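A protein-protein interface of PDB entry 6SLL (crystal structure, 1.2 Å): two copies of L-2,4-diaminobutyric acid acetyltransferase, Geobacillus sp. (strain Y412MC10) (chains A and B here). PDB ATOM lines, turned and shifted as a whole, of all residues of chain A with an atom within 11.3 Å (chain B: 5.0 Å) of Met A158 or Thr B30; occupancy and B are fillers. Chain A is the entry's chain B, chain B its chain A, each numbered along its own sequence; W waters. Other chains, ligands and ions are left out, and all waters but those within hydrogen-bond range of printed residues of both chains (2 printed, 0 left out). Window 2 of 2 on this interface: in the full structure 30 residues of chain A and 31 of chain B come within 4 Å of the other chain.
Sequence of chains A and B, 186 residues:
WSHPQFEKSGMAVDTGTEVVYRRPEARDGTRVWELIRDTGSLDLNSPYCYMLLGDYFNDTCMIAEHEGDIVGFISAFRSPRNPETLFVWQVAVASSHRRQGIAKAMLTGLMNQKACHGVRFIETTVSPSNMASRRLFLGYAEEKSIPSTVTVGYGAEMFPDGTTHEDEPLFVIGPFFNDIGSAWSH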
ATOM      1  N   ASP A  43     -10.707  -6.657  -0.447  1.00  0.00           N
ATOM      2  CA  ASP A  43     -10.184  -7.024   0.889  1.00  0.00           C
ATOM      3  C   ASP A  43      -9.072  -6.050   1.331  1.00  0.00           C
ATOM      4  O   ASP A  43      -7.966  -5.966   0.743  1.00  0.00           O
ATOM      5  CB  ASP A  43      -9.643  -8.382   0.877  1.00  0.00           C
ATOM      6  CG  ASP A  43     -10.646  -9.473   0.455  1.00  0.00           C
ATOM      7  OD1 ASP A  43     -11.806  -9.338   0.832  1.00  0.00           O
ATOM      8  OD2 ASP A  43     -10.182 -10.387  -0.231  1.00  0.00           O
ATOM      9  N   THR A 125      -7.376 -12.189 -10.120  1.00  0.00           N
ATOM     10  CA  THR A 125      -8.545 -12.999  -9.734  1.00  0.00           C
ATOM     11  C   THR A 125      -9.760 -12.092  -9.618  1.00  0.00           C
ATOM     12  O   THR A 125      -9.664 -10.921  -9.223  1.00  0.00           O
ATOM     13  CB  THR A 125      -8.298 -13.747  -8.417  1.00  0.00           C
ATOM     14  OG1 THR A 125      -8.267 -12.868  -7.282  1.00  0.00           O
ATOM     15  CG2 THR A 125      -7.122 -14.623  -8.453  1.00  0.00           C
ATOM     16  N   THR A 151      -9.114 -20.296 -14.603  1.00  0.00           N
ATOM     17  CA  THR A 151      -8.852 -21.520 -13.808  1.00  0.00           C
ATOM     18  C   THR A 151      -9.251 -21.222 -12.368  1.00  0.00           C
ATOM     19  O   THR A 151      -9.759 -20.167 -12.015  1.00  0.00           O
ATOM     20  CB  THR A 151      -7.406 -21.909 -13.923  1.00  0.00           C
ATOM     21  OG1 THR A 151      -6.532 -20.847 -13.535  1.00  0.00           O
ATOM     22  CG2 THR A 151      -7.091 -22.429 -15.296  1.00  0.00           C
ATOM     23  N   VAL A 152      -9.145 -22.302 -11.532  1.00  0.00           N
ATOM     24  CA  VAL A 152      -9.697 -22.334 -10.212  1.00  0.00           C
ATOM     25  C   VAL A 152      -9.332 -21.101  -9.241  1.00  0.00           C
ATOM     26  O   VAL A 152     -10.171 -20.674  -8.477  1.00  0.00           O
ATOM     27  CB  VAL A 152      -9.538 -23.679  -9.519  1.00  0.00           C
ATOM     28  CG1 VAL A 152      -8.119 -23.977  -9.117  1.00  0.00           C
ATOM     29  CG2 VAL A 152     -10.409 -23.778  -8.348  1.00  0.00           C
ATOM     30  N   GLY A 153      -8.128 -20.716  -9.274  1.00  0.00           N
ATOM     31  CA  GLY A 153      -7.693 -19.667  -8.362  1.00  0.00           C
ATOM     32  C   GLY A 153      -7.807 -20.064  -6.903  1.00  0.00           C
ATOM     33  O   GLY A 153      -7.488 -21.205  -6.601  1.00  0.00           O
ATOM     34  N   TYR A 154      -8.182 -19.137  -6.046  1.00  0.00           N
ATOM     35  CA  TYR A 154      -8.258 -19.389  -4.628  1.00  0.00           C
ATOM     36  C   TYR A 154      -9.767 -19.567  -4.258  1.00  0.00           C
ATOM     37  O   TYR A 154     -10.535 -18.608  -4.226  1.00  0.00           O
ATOM     38  CB  TYR A 154      -7.650 -18.261  -3.801  1.00  0.00           C
ATOM     39  CG  TYR A 154      -6.276 -17.816  -4.242  1.00  0.00           C
ATOM     40  CD1 TYR A 154      -5.299 -18.705  -4.525  1.00  0.00           C
ATOM     41  CD2 TYR A 154      -5.963 -16.465  -4.326  1.00  0.00           C
ATOM     42  CE1 TYR A 154      -4.020 -18.279  -4.862  1.00  0.00           C
ATOM     43  CE2 TYR A 154      -4.719 -16.044  -4.704  1.00  0.00           C
ATOM     44  CZ  TYR A 154      -3.738 -16.945  -4.996  1.00  0.00           C
ATOM     45  OH  TYR A 154      -2.519 -16.443  -5.409  1.00  0.00           O
ATOM     46  N   GLY A 155     -10.134 -20.836  -3.951  1.00  0.00           N
ATOM     47  CA  GLY A 155     -11.534 -21.105  -3.626  1.00  0.00           C
ATOM     48  C   GLY A 155     -11.880 -20.563  -2.245  1.00  0.00           C
ATOM     49  O   GLY A 155     -11.045 -20.361  -1.404  1.00  0.00           O
ATOM     50  N   ALA A 156     -13.224 -20.416  -2.041  1.00  0.00           N
ATOM     51  CA  ALA A 156     -13.727 -19.950  -0.798  1.00  0.00           C
ATOM     52  C   ALA A 156     -13.196 -20.679   0.378  1.00  0.00           C
ATOM     53  O   ALA A 156     -13.035 -20.129   1.463  1.00  0.00           O
ATOM     54  CB  ALA A 156     -15.232 -20.047  -0.856  1.00  0.00           C
ATOM     55  N   GLU A 157     -12.978 -22.020   0.259  1.00  0.00           N
ATOM     56  CA  GLU A 157     -12.528 -22.843   1.334  1.00  0.00           C
ATOM     57  C   GLU A 157     -11.193 -22.499   1.868  1.00  0.00           C
ATOM     58  O   GLU A 157     -10.796 -22.975   2.903  1.00  0.00           O
ATOM     59  CB  GLU A 157     -12.560 -24.332   0.901  1.00  0.00           C
ATOM     60  CG  GLU A 157     -11.611 -24.690  -0.254  1.00  0.00           C
ATOM     61  CD  GLU A 157     -12.140 -24.465  -1.689  1.00  0.00           C
ATOM     62  OE1 GLU A 157     -13.195 -23.806  -1.876  1.00  0.00           O
ATOM     63  OE2 GLU A 157     -11.408 -25.060  -2.560  1.00  0.00           O
ATOM     64  N   MET A 158     -10.408 -21.727   1.046  1.00  0.00           N
ATOM     65  CA  MET A 158      -9.066 -21.376   1.497  1.00  0.00           C
ATOM     66  C   MET A 158      -9.061 -20.262   2.531  1.00  0.00           C
ATOM     67  O   MET A 158      -8.045 -20.015   3.135  1.00  0.00           O
ATOM     68  CB  MET A 158      -8.171 -20.887   0.291  1.00  0.00           C
ATOM     69  CG  MET A 158      -7.915 -22.067  -0.680  1.00  0.00           C
ATOM     70  SD  MET A 158      -6.871 -21.601  -2.093  1.00  0.00           S
ATOM     71  CE  MET A 158      -5.417 -20.960  -1.327  1.00  0.00           C
ATOM     72  N   PHE A 159     -10.180 -19.559   2.686  1.00  0.00           N
ATOM     73  CA  PHE A 159     -10.265 -18.341   3.455  1.00  0.00           C
ATOM     74  C   PHE A 159     -10.536 -18.694   4.943  1.00  0.00           C
ATOM     75  O   PHE A 159     -10.961 -19.806   5.233  1.00  0.00           O
ATOM     76  CB  PHE A 159     -11.209 -17.372   2.857  1.00  0.00           C
ATOM     77  CG  PHE A 159     -10.736 -16.809   1.590  1.00  0.00           C
ATOM     78  CD1 PHE A 159     -10.818 -17.470   0.426  1.00  0.00           C
ATOM     79  CD2 PHE A 159     -10.051 -15.573   1.558  1.00  0.00           C
ATOM     80  CE1 PHE A 159     -10.279 -17.002  -0.803  1.00  0.00           C
ATOM     81  CE2 PHE A 159      -9.479 -15.110   0.414  1.00  0.00           C
ATOM     82  CZ  PHE A 159      -9.604 -15.782  -0.764  1.00  0.00           C
ATOM     83  N   PRO A 160     -10.402 -17.757   5.861  1.00  0.00           N
ATOM     84  CA  PRO A 160     -10.565 -18.113   7.304  1.00  0.00           C
ATOM     85  C   PRO A 160     -11.946 -18.446   7.701  1.00  0.00           C
ATOM     86  O   PRO A 160     -12.940 -18.029   7.090  1.00  0.00           O
ATOM     87  CB  PRO A 160     -10.182 -16.845   8.046  1.00  0.00           C
ATOM     88  CG  PRO A 160      -9.214 -16.145   7.096  1.00  0.00           C
ATOM     89  CD  PRO A 160      -9.763 -16.453   5.716  1.00  0.00           C
ATOM     90  N   ASP A 161     -11.993 -19.367   8.673  1.00  0.00           N
ATOM     91  CA  ASP A 161     -13.251 -19.825   9.264  1.00  0.00           C
ATOM     92  C   ASP A 161     -14.064 -18.699   9.750  1.00  0.00           C
ATOM     93  O   ASP A 161     -13.540 -17.760  10.276  1.00  0.00           O
ATOM     94  CB  ASP A 161     -12.979 -20.766  10.481  1.00  0.00           C
ATOM     95  CG  ASP A 161     -12.544 -22.146  10.000  1.00  0.00           C
ATOM     96  OD1 ASP A 161     -12.698 -22.342   8.761  1.00  0.00           O
ATOM     97  OD2 ASP A 161     -12.075 -22.962  10.841  1.00  0.00           O
ATOM     98  N   GLY A 162     -15.384 -18.878   9.744  1.00  0.00           N
ATOM     99  CA  GLY A 162     -16.149 -17.866  10.423  1.00  0.00           C
ATOM    100  C   GLY A 162     -16.246 -16.460   9.842  1.00  0.00           C
ATOM    101  O   GLY A 162     -16.817 -15.551  10.465  1.00  0.00           O
ATOM    102  N   THR A 163     -15.784 -16.201   8.674  1.00  0.00           N
ATOM    103  CA  THR A 163     -16.572 -15.327   7.791  1.00  0.00           C
ATOM    104  C   THR A 163     -16.482 -16.042   6.411  1.00  0.00           C
ATOM    105  O   THR A 163     -16.045 -17.174   6.268  1.00  0.00           O
ATOM    106  CB  THR A 163     -16.057 -13.890   7.742  1.00  0.00           C
ATOM    107  OG1 THR A 163     -14.652 -14.080   7.513  1.00  0.00           O
ATOM    108  CG2 THR A 163     -16.302 -13.020   9.181  1.00  0.00           C
ATOM    109  N   THR A 164     -17.285 -15.529   5.509  1.00  0.00           N
ATOM    110  CA  THR A 164     -17.577 -16.102   4.190  1.00  0.00           C
ATOM    111  C   THR A 164     -16.789 -15.231   3.184  1.00  0.00           C
ATOM    112  O   THR A 164     -16.860 -13.984   3.327  1.00  0.00           O
ATOM    113  CB  THR A 164     -19.118 -15.954   3.946  1.00  0.00           C
ATOM    114  OG1 THR A 164     -19.816 -16.761   4.904  1.00  0.00           O
ATOM    115  CG2 THR A 164     -19.529 -16.406   2.544  1.00  0.00           C
ATOM    116  N   HIS A 165     -16.002 -15.830   2.328  1.00  0.00           N
ATOM    117  CA  HIS A 165     -15.354 -15.126   1.264  1.00  0.00           C
ATOM    118  C   HIS A 165     -15.761 -15.848   0.000  1.00  0.00           C
ATOM    119  O   HIS A 165     -15.833 -17.096  -0.040  1.00  0.00           O
ATOM    120  CB  HIS A 165     -13.838 -15.182   1.399  1.00  0.00           C
ATOM    121  CG  HIS A 165     -13.075 -14.208   0.572  1.00  0.00           C
ATOM    122  ND1 HIS A 165     -12.893 -14.327  -0.787  1.00  0.00           N
ATOM    123  CD2 HIS A 165     -12.462 -13.073   0.929  1.00  0.00           C
ATOM    124  CE1 HIS A 165     -12.160 -13.303  -1.231  1.00  0.00           C
ATOM    125  NE2 HIS A 165     -11.883 -12.517  -0.201  1.00  0.00           N
ATOM    126  N   GLU A 166     -15.934 -15.140  -1.073  1.00  0.00           N
ATOM    127  CA  GLU A 166     -16.198 -15.678  -2.348  1.00  0.00           C
ATOM    128  C   GLU A 166     -14.995 -16.418  -2.965  1.00  0.00           C
ATOM    129  O   GLU A 166     -13.839 -16.115  -2.585  1.00  0.00           O
ATOM    130  CB  GLU A 166     -16.706 -14.694  -3.382  1.00  0.00           C
ATOM    131  CG  GLU A 166     -18.084 -14.030  -3.090  1.00  0.00           C
ATOM    132  CD  GLU A 166     -18.244 -12.923  -4.210  1.00  0.00           C
ATOM    133  OE1 GLU A 166     -18.174 -11.688  -3.920  1.00  0.00           O
ATOM    134  OE2 GLU A 166     -18.597 -13.330  -5.413  1.00  0.00           O
ATOM    135  N   ASP A 167     -15.224 -17.326  -3.886  1.00  0.00           N
ATOM    136  CA  ASP A 167     -14.152 -17.827  -4.701  1.00  0.00           C
ATOM    137  C   ASP A 167     -13.465 -16.669  -5.435  1.00  0.00           C
ATOM    138  O   ASP A 167     -14.039 -15.679  -5.815  1.00  0.00           O
ATOM    139  CB  ASP A 167     -14.653 -18.782  -5.813  1.00  0.00           C
ATOM    140  CG  ASP A 167     -15.286 -20.111  -5.312  1.00  0.00           C
ATOM    141  OD1 ASP A 167     -14.970 -20.503  -4.221  1.00  0.00           O
ATOM    142  OD2 ASP A 167     -16.110 -20.651  -6.050  1.00  0.00           O
ATOM    143  N   GLU A 168     -12.163 -16.907  -5.707  1.00  0.00           N
ATOM    144  CA  GLU A 168     -11.279 -15.945  -6.440  1.00  0.00           C
ATOM    145  C   GLU A 168     -10.700 -16.702  -7.659  1.00  0.00           C
ATOM    146  O   GLU A 168      -9.519 -17.040  -7.643  1.00  0.00           O
ATOM    147  CB  GLU A 168     -10.179 -15.452  -5.532  1.00  0.00           C
ATOM    148  CG  GLU A 168     -10.688 -14.496  -4.473  1.00  0.00           C
ATOM    149  CD  GLU A 168     -10.902 -13.061  -4.904  1.00  0.00           C
ATOM    150  OE1 GLU A 168     -10.611 -12.710  -6.075  1.00  0.00           O
ATOM    151  OE2 GLU A 168     -11.326 -12.267  -4.032  1.00  0.00           O
ATOM    152  N   PRO A 169     -11.479 -16.959  -8.695  1.00  0.00           N
ATOM    153  CA  PRO A 169     -10.952 -17.680  -9.851  1.00  0.00           C
ATOM    154  C   PRO A 169      -9.894 -16.820 -10.552  1.00  0.00           C
ATOM    155  O   PRO A 169      -9.959 -15.580 -10.589  1.00  0.00           O
ATOM    156  CB  PRO A 169     -12.146 -17.869 -10.734  1.00  0.00           C
ATOM    157  CG  PRO A 169     -13.111 -16.925 -10.207  1.00  0.00           C
ATOM    158  CD  PRO A 169     -12.893 -16.641  -8.833  1.00  0.00           C
ATOM    159  N   LEU A 170      -8.924 -17.504 -11.144  1.00  0.00           N
ATOM    160  CA  LEU A 170      -7.788 -16.862 -11.841  1.00  0.00           C
ATOM    161  C   LEU A 170      -8.047 -16.652 -13.299  1.00  0.00           C
ATOM    162  O   LEU A 170      -8.314 -17.604 -14.037  1.00  0.00           O
ATOM    163  CB  LEU A 170      -6.510 -17.723 -11.645  1.00  0.00           C
ATOM    164  CG  LEU A 170      -5.261 -17.176 -12.208  1.00  0.00           C
ATOM    165  CD1 LEU A 170      -4.796 -15.920 -11.466  1.00  0.00           C
ATOM    166  CD2 LEU A 170      -4.174 -18.249 -12.231  1.00  0.00           C
ATOM    167  N   ALA B  26       0.383 -20.984  -1.275  1.00  0.00           N
ATOM    168  CA  ALA B  26      -0.858 -20.217  -1.176  1.00  0.00           C
ATOM    169  C   ALA B  26      -1.777 -20.741  -0.086  1.00  0.00           C
ATOM    170  O   ALA B  26      -2.465 -19.999   0.577  1.00  0.00           O
ATOM    171  CB  ALA B  26      -1.561 -20.173  -2.511  1.00  0.00           C
ATOM    172  N   ARG B  27      -1.834 -22.094   0.011  1.00  0.00           N
ATOM    173  CA  ARG B  27      -2.767 -22.686   1.008  1.00  0.00           C
ATOM    174  C   ARG B  27      -2.440 -22.382   2.440  1.00  0.00           C
ATOM    175  O   ARG B  27      -3.281 -22.619   3.261  1.00  0.00           O
ATOM    176  CB  ARG B  27      -2.852 -24.195   0.776  1.00  0.00           C
ATOM    177  CG  ARG B  27      -1.511 -24.953   0.927  1.00  0.00           C
ATOM    178  CD  ARG B  27      -1.360 -26.412   0.486  1.00  0.00           C
ATOM    179  NE  ARG B  27      -1.837 -27.294   1.487  1.00  0.00           N
ATOM    180  CZ  ARG B  27      -1.601 -28.579   1.602  1.00  0.00           C
ATOM    181  NH1 ARG B  27      -2.138 -29.201   2.645  1.00  0.00           N
ATOM    182  NH2 ARG B  27      -0.766 -29.128   0.723  1.00  0.00           N
ATOM    183  N   ASP B  28      -1.242 -21.868   2.680  1.00  0.00           N
ATOM    184  CA  ASP B  28      -0.900 -21.449   4.038  1.00  0.00           C
ATOM    185  C   ASP B  28      -1.456 -20.053   4.410  1.00  0.00           C
ATOM    186  O   ASP B  28      -1.273 -19.619   5.541  1.00  0.00           O
ATOM    187  CB  ASP B  28       0.597 -21.421   4.233  1.00  0.00           C
ATOM    188  CG  ASP B  28       1.207 -22.753   4.037  1.00  0.00           C
ATOM    189  OD1 ASP B  28       0.771 -23.747   4.714  1.00  0.00           O
ATOM    190  OD2 ASP B  28       2.211 -22.903   3.324  1.00  0.00           O
ATOM    191  N   GLY B  29      -2.097 -19.374   3.429  1.00  0.00           N
ATOM    192  CA  GLY B  29      -2.440 -17.972   3.680  1.00  0.00           C
ATOM    193  C   GLY B  29      -3.284 -17.764   4.958  1.00  0.00           C
ATOM    194  O   GLY B  29      -2.980 -16.859   5.712  1.00  0.00           O
ATOM    195  N   THR B  30      -4.323 -18.591   5.144  1.00  0.00           N
ATOM    196  CA  THR B  30      -5.173 -18.412   6.339  1.00  0.00           C
ATOM    197  C   THR B  30      -4.371 -18.620   7.589  1.00  0.00           C
ATOM    198  O   THR B  30      -4.558 -17.842   8.544  1.00  0.00           O
ATOM    199  CB  THR B  30      -6.400 -19.276   6.188  1.00  0.00           C
ATOM    200  OG1 THR B  30      -7.297 -18.601   5.299  1.00  0.00           O
ATOM    201  CG2 THR B  30      -7.066 -19.548   7.543  1.00  0.00           C
ATOM    202  N   ARG B  31      -3.629 -19.707   7.681  1.00  0.00           N
ATOM    203  CA  ARG B  31      -2.894 -19.969   8.898  1.00  0.00           C
ATOM    204  C   ARG B  31      -1.808 -18.917   9.215  1.00  0.00           C
ATOM    205  O   ARG B  31      -1.558 -18.577  10.389  1.00  0.00           O
ATOM    206  CB  ARG B  31      -2.421 -21.360   9.017  1.00  0.00           C
ATOM    207  CG  ARG B  31      -3.521 -22.391   9.094  1.00  0.00           C
ATOM    208  CD  ARG B  31      -3.048 -23.808   8.846  1.00  0.00           C
ATOM    209  NE  ARG B  31      -2.405 -24.233  10.017  1.00  0.00           N
ATOM    210  CZ  ARG B  31      -1.366 -25.033   9.971  1.00  0.00           C
ATOM    211  NH1 ARG B  31      -0.796 -25.407  11.100  1.00  0.00           N
ATOM    212  NH2 ARG B  31      -0.982 -25.488   8.786  1.00  0.00           N
ATOM    213  N   VAL B  32      -1.188 -18.422   8.165  1.00  0.00           N
ATOM    214  CA  VAL B  32      -0.247 -17.294   8.351  1.00  0.00           C
ATOM    215  C   VAL B  32      -0.991 -16.021   8.807  1.00  0.00           C
ATOM    216  O   VAL B  32      -0.531 -15.360   9.761  1.00  0.00           O
ATOM    217  CB  VAL B  32       0.531 -17.056   7.019  1.00  0.00           C
ATOM    218  CG1 VAL B  32       1.311 -15.726   7.079  1.00  0.00           C
ATOM    219  CG2 VAL B  32       1.469 -18.214   6.738  1.00  0.00           C
ATOM    220  N   TRP B  33      -2.130 -15.741   8.174  1.00  0.00           N
ATOM    221  CA  TRP B  33      -2.937 -14.593   8.611  1.00  0.00           C
ATOM    222  C   TRP B  33      -3.245 -14.704  10.096  1.00  0.00           C
ATOM    223  O   TRP B  33      -3.185 -13.731  10.862  1.00  0.00           O
ATOM    224  CB  TRP B  33      -4.169 -14.540   7.702  1.00  0.00           C
ATOM    225  CG  TRP B  33      -5.139 -13.425   8.035  1.00  0.00           C
ATOM    226  CD1 TRP B  33      -5.097 -12.152   7.634  1.00  0.00           C
ATOM    227  CD2 TRP B  33      -6.303 -13.564   8.892  1.00  0.00           C
ATOM    228  NE1 TRP B  33      -6.150 -11.459   8.167  1.00  0.00           N
ATOM    229  CE2 TRP B  33      -6.924 -12.292   8.914  1.00  0.00           C
ATOM    230  CE3 TRP B  33      -6.930 -14.683   9.547  1.00  0.00           C
ATOM    231  CZ2 TRP B  33      -8.103 -12.045   9.589  1.00  0.00           C
ATOM    232  CZ3 TRP B  33      -8.109 -14.397  10.172  1.00  0.00           C
ATOM    233  CH2 TRP B  33      -8.685 -13.146  10.200  1.00  0.00           C
ATOM    234  N   GLU B  34      -3.695 -15.909  10.506  1.00  0.00           N
ATOM    235  CA  GLU B  34      -4.036 -16.095  11.920  1.00  0.00           C
ATOM    236  C   GLU B  34      -2.820 -15.898  12.852  1.00  0.00           C
ATOM    237  O   GLU B  34      -2.969 -15.292  13.899  1.00  0.00           O
ATOM    238  CB  GLU B  34      -4.629 -17.517  12.115  1.00  0.00           C
ATOM    239  CG  GLU B  34      -6.016 -17.654  11.483  1.00  0.00           C
ATOM    240  CD  GLU B  34      -6.663 -19.014  11.484  1.00  0.00           C
ATOM    241  OE1 GLU B  34      -5.871 -20.024  11.492  1.00  0.00           O
ATOM    242  OE2 GLU B  34      -7.912 -19.120  11.311  1.00  0.00           O
ATOM    243  N   PRO B  47      -6.276 -11.927   4.399  1.00  0.00           N
ATOM    244  CA  PRO B  47      -5.892 -13.274   4.122  1.00  0.00           C
ATOM    245  C   PRO B  47      -5.384 -13.466   2.685  1.00  0.00           C
ATOM    246  O   PRO B  47      -4.353 -14.160   2.452  1.00  0.00           O
ATOM    247  CB  PRO B  47      -7.165 -14.094   4.437  1.00  0.00           C
ATOM    248  CG  PRO B  47      -7.873 -13.238   5.452  1.00  0.00           C
ATOM    249  CD  PRO B  47      -7.577 -11.801   5.063  1.00  0.00           C
ATOM    250  N   MET B  51      -2.001 -15.292   0.949  1.00  0.00           N
ATOM    251  CA  MET B  51      -2.047 -16.251  -0.153  1.00  0.00           C
ATOM    252  C   MET B  51      -1.146 -15.839  -1.302  1.00  0.00           C
ATOM    253  O   MET B  51      -0.398 -16.648  -1.843  1.00  0.00           O
ATOM    254  CB  MET B  51      -3.479 -16.408  -0.663  1.00  0.00           C
ATOM    255  CG  MET B  51      -4.415 -16.978   0.392  1.00  0.00           C
ATOM    256  SD  MET B  51      -6.121 -16.972  -0.251  1.00  0.00           S
ATOM    257  CE  MET B  51      -6.987 -17.333   1.268  1.00  0.00           C
HETATM  258  O   HOH W   1      -5.209 -20.229   2.891  1.00  0.00           O
HETATM  259  O   HOH W   2      -9.680 -20.497   9.826  1.00  0.00           O
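The side-chain hydroxyl of Thr B30 sits at hydrogen-bond distance from the backbone carbonyl oxygen of Met A158 (2.7 Å). N of Pro A160 sits close to OG1 of Thr B30, at 3.3 Å.
The backbone carbonyl oxygen of Tyr A154 sits at hydrogen-bond distance from the backbone NH of Glu A168, at 2.8 Å.
Among the printed residues, merely in contact across the chains: Tyr A154 with Ala B26 (3.9 Å), Met A158 with Ala B26 (3.6 Å), Met A158 with Arg B27 (3.9 Å), Met A158 with Met B51 (3.4 Å), Phe A159 with Thr B30 (3.3 Å), Phe A159 with Met B51 (3.4 Å), Pro A160 with Trp B33 (3.7 Å) and Pro A160 with Pro B47 (3.6 Å).
Printed residues of chain B within 4 Å of Tyr A154: Ala B26. Met A158 touches just these residues of chain B: Ala B26, Arg B27, Thr B30 and Met B51. Printed residues of chain A within 4 Å of Arg B27: Met A158. No residue of chain A comes within 4 Å of Gly B29. Printed residues of chain A within 4 Å of Thr B30: Met A158, Phe A159 and Pro A160. Val B32 touches none of the printed residues of chain A. Of the printed residues of chain A, Trp B33 touches Pro A160. No residue of chain A comes within 4 Å of Glu B34. Of chain A, only Pro A160 comes within 4 Å of Pro B47. Met B51 touches two residues of chain A. The nearest printed residue of chain B that does not touch Met A158 is Gly B29 (5.6 Å). The nearest residue of chain A that does not touch Thr B30 is Asp A161 (5.1 Å).
Of the 22 printed residues of chain A, 4 touch a printed residue of chain B. Along chain A the printed residues that touch a printed residue of chain B span positions 154 to 160. Printed residues of chain B that touch a printed residue of chain A: Ala B26, Arg B27, Thr B30, Trp B33, Pro B47 and Met B51. Hydrophobic or aromatic side chains of chain B within 4 Å of the printed part of chain A: Ala B26, Trp B33, Pro B47 and Met B51. Among the printed residues, 10 pairs touch across the chains.
No position is printed for both chains.
Water W2 lies within hydrogen-bond range of the side-chain carboxylate (OE2) of Glu B34 (2.7 Å) and the backbone NH (N) of Asp A161 (2.8 Å). Water W1 lies within hydrogen-bond range of O of Met A158 (2.9 Å), N of Thr B30 (2.9 Å), O of Arg B27 (3.1 Å) and N of Gly B29 (3.3 Å).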
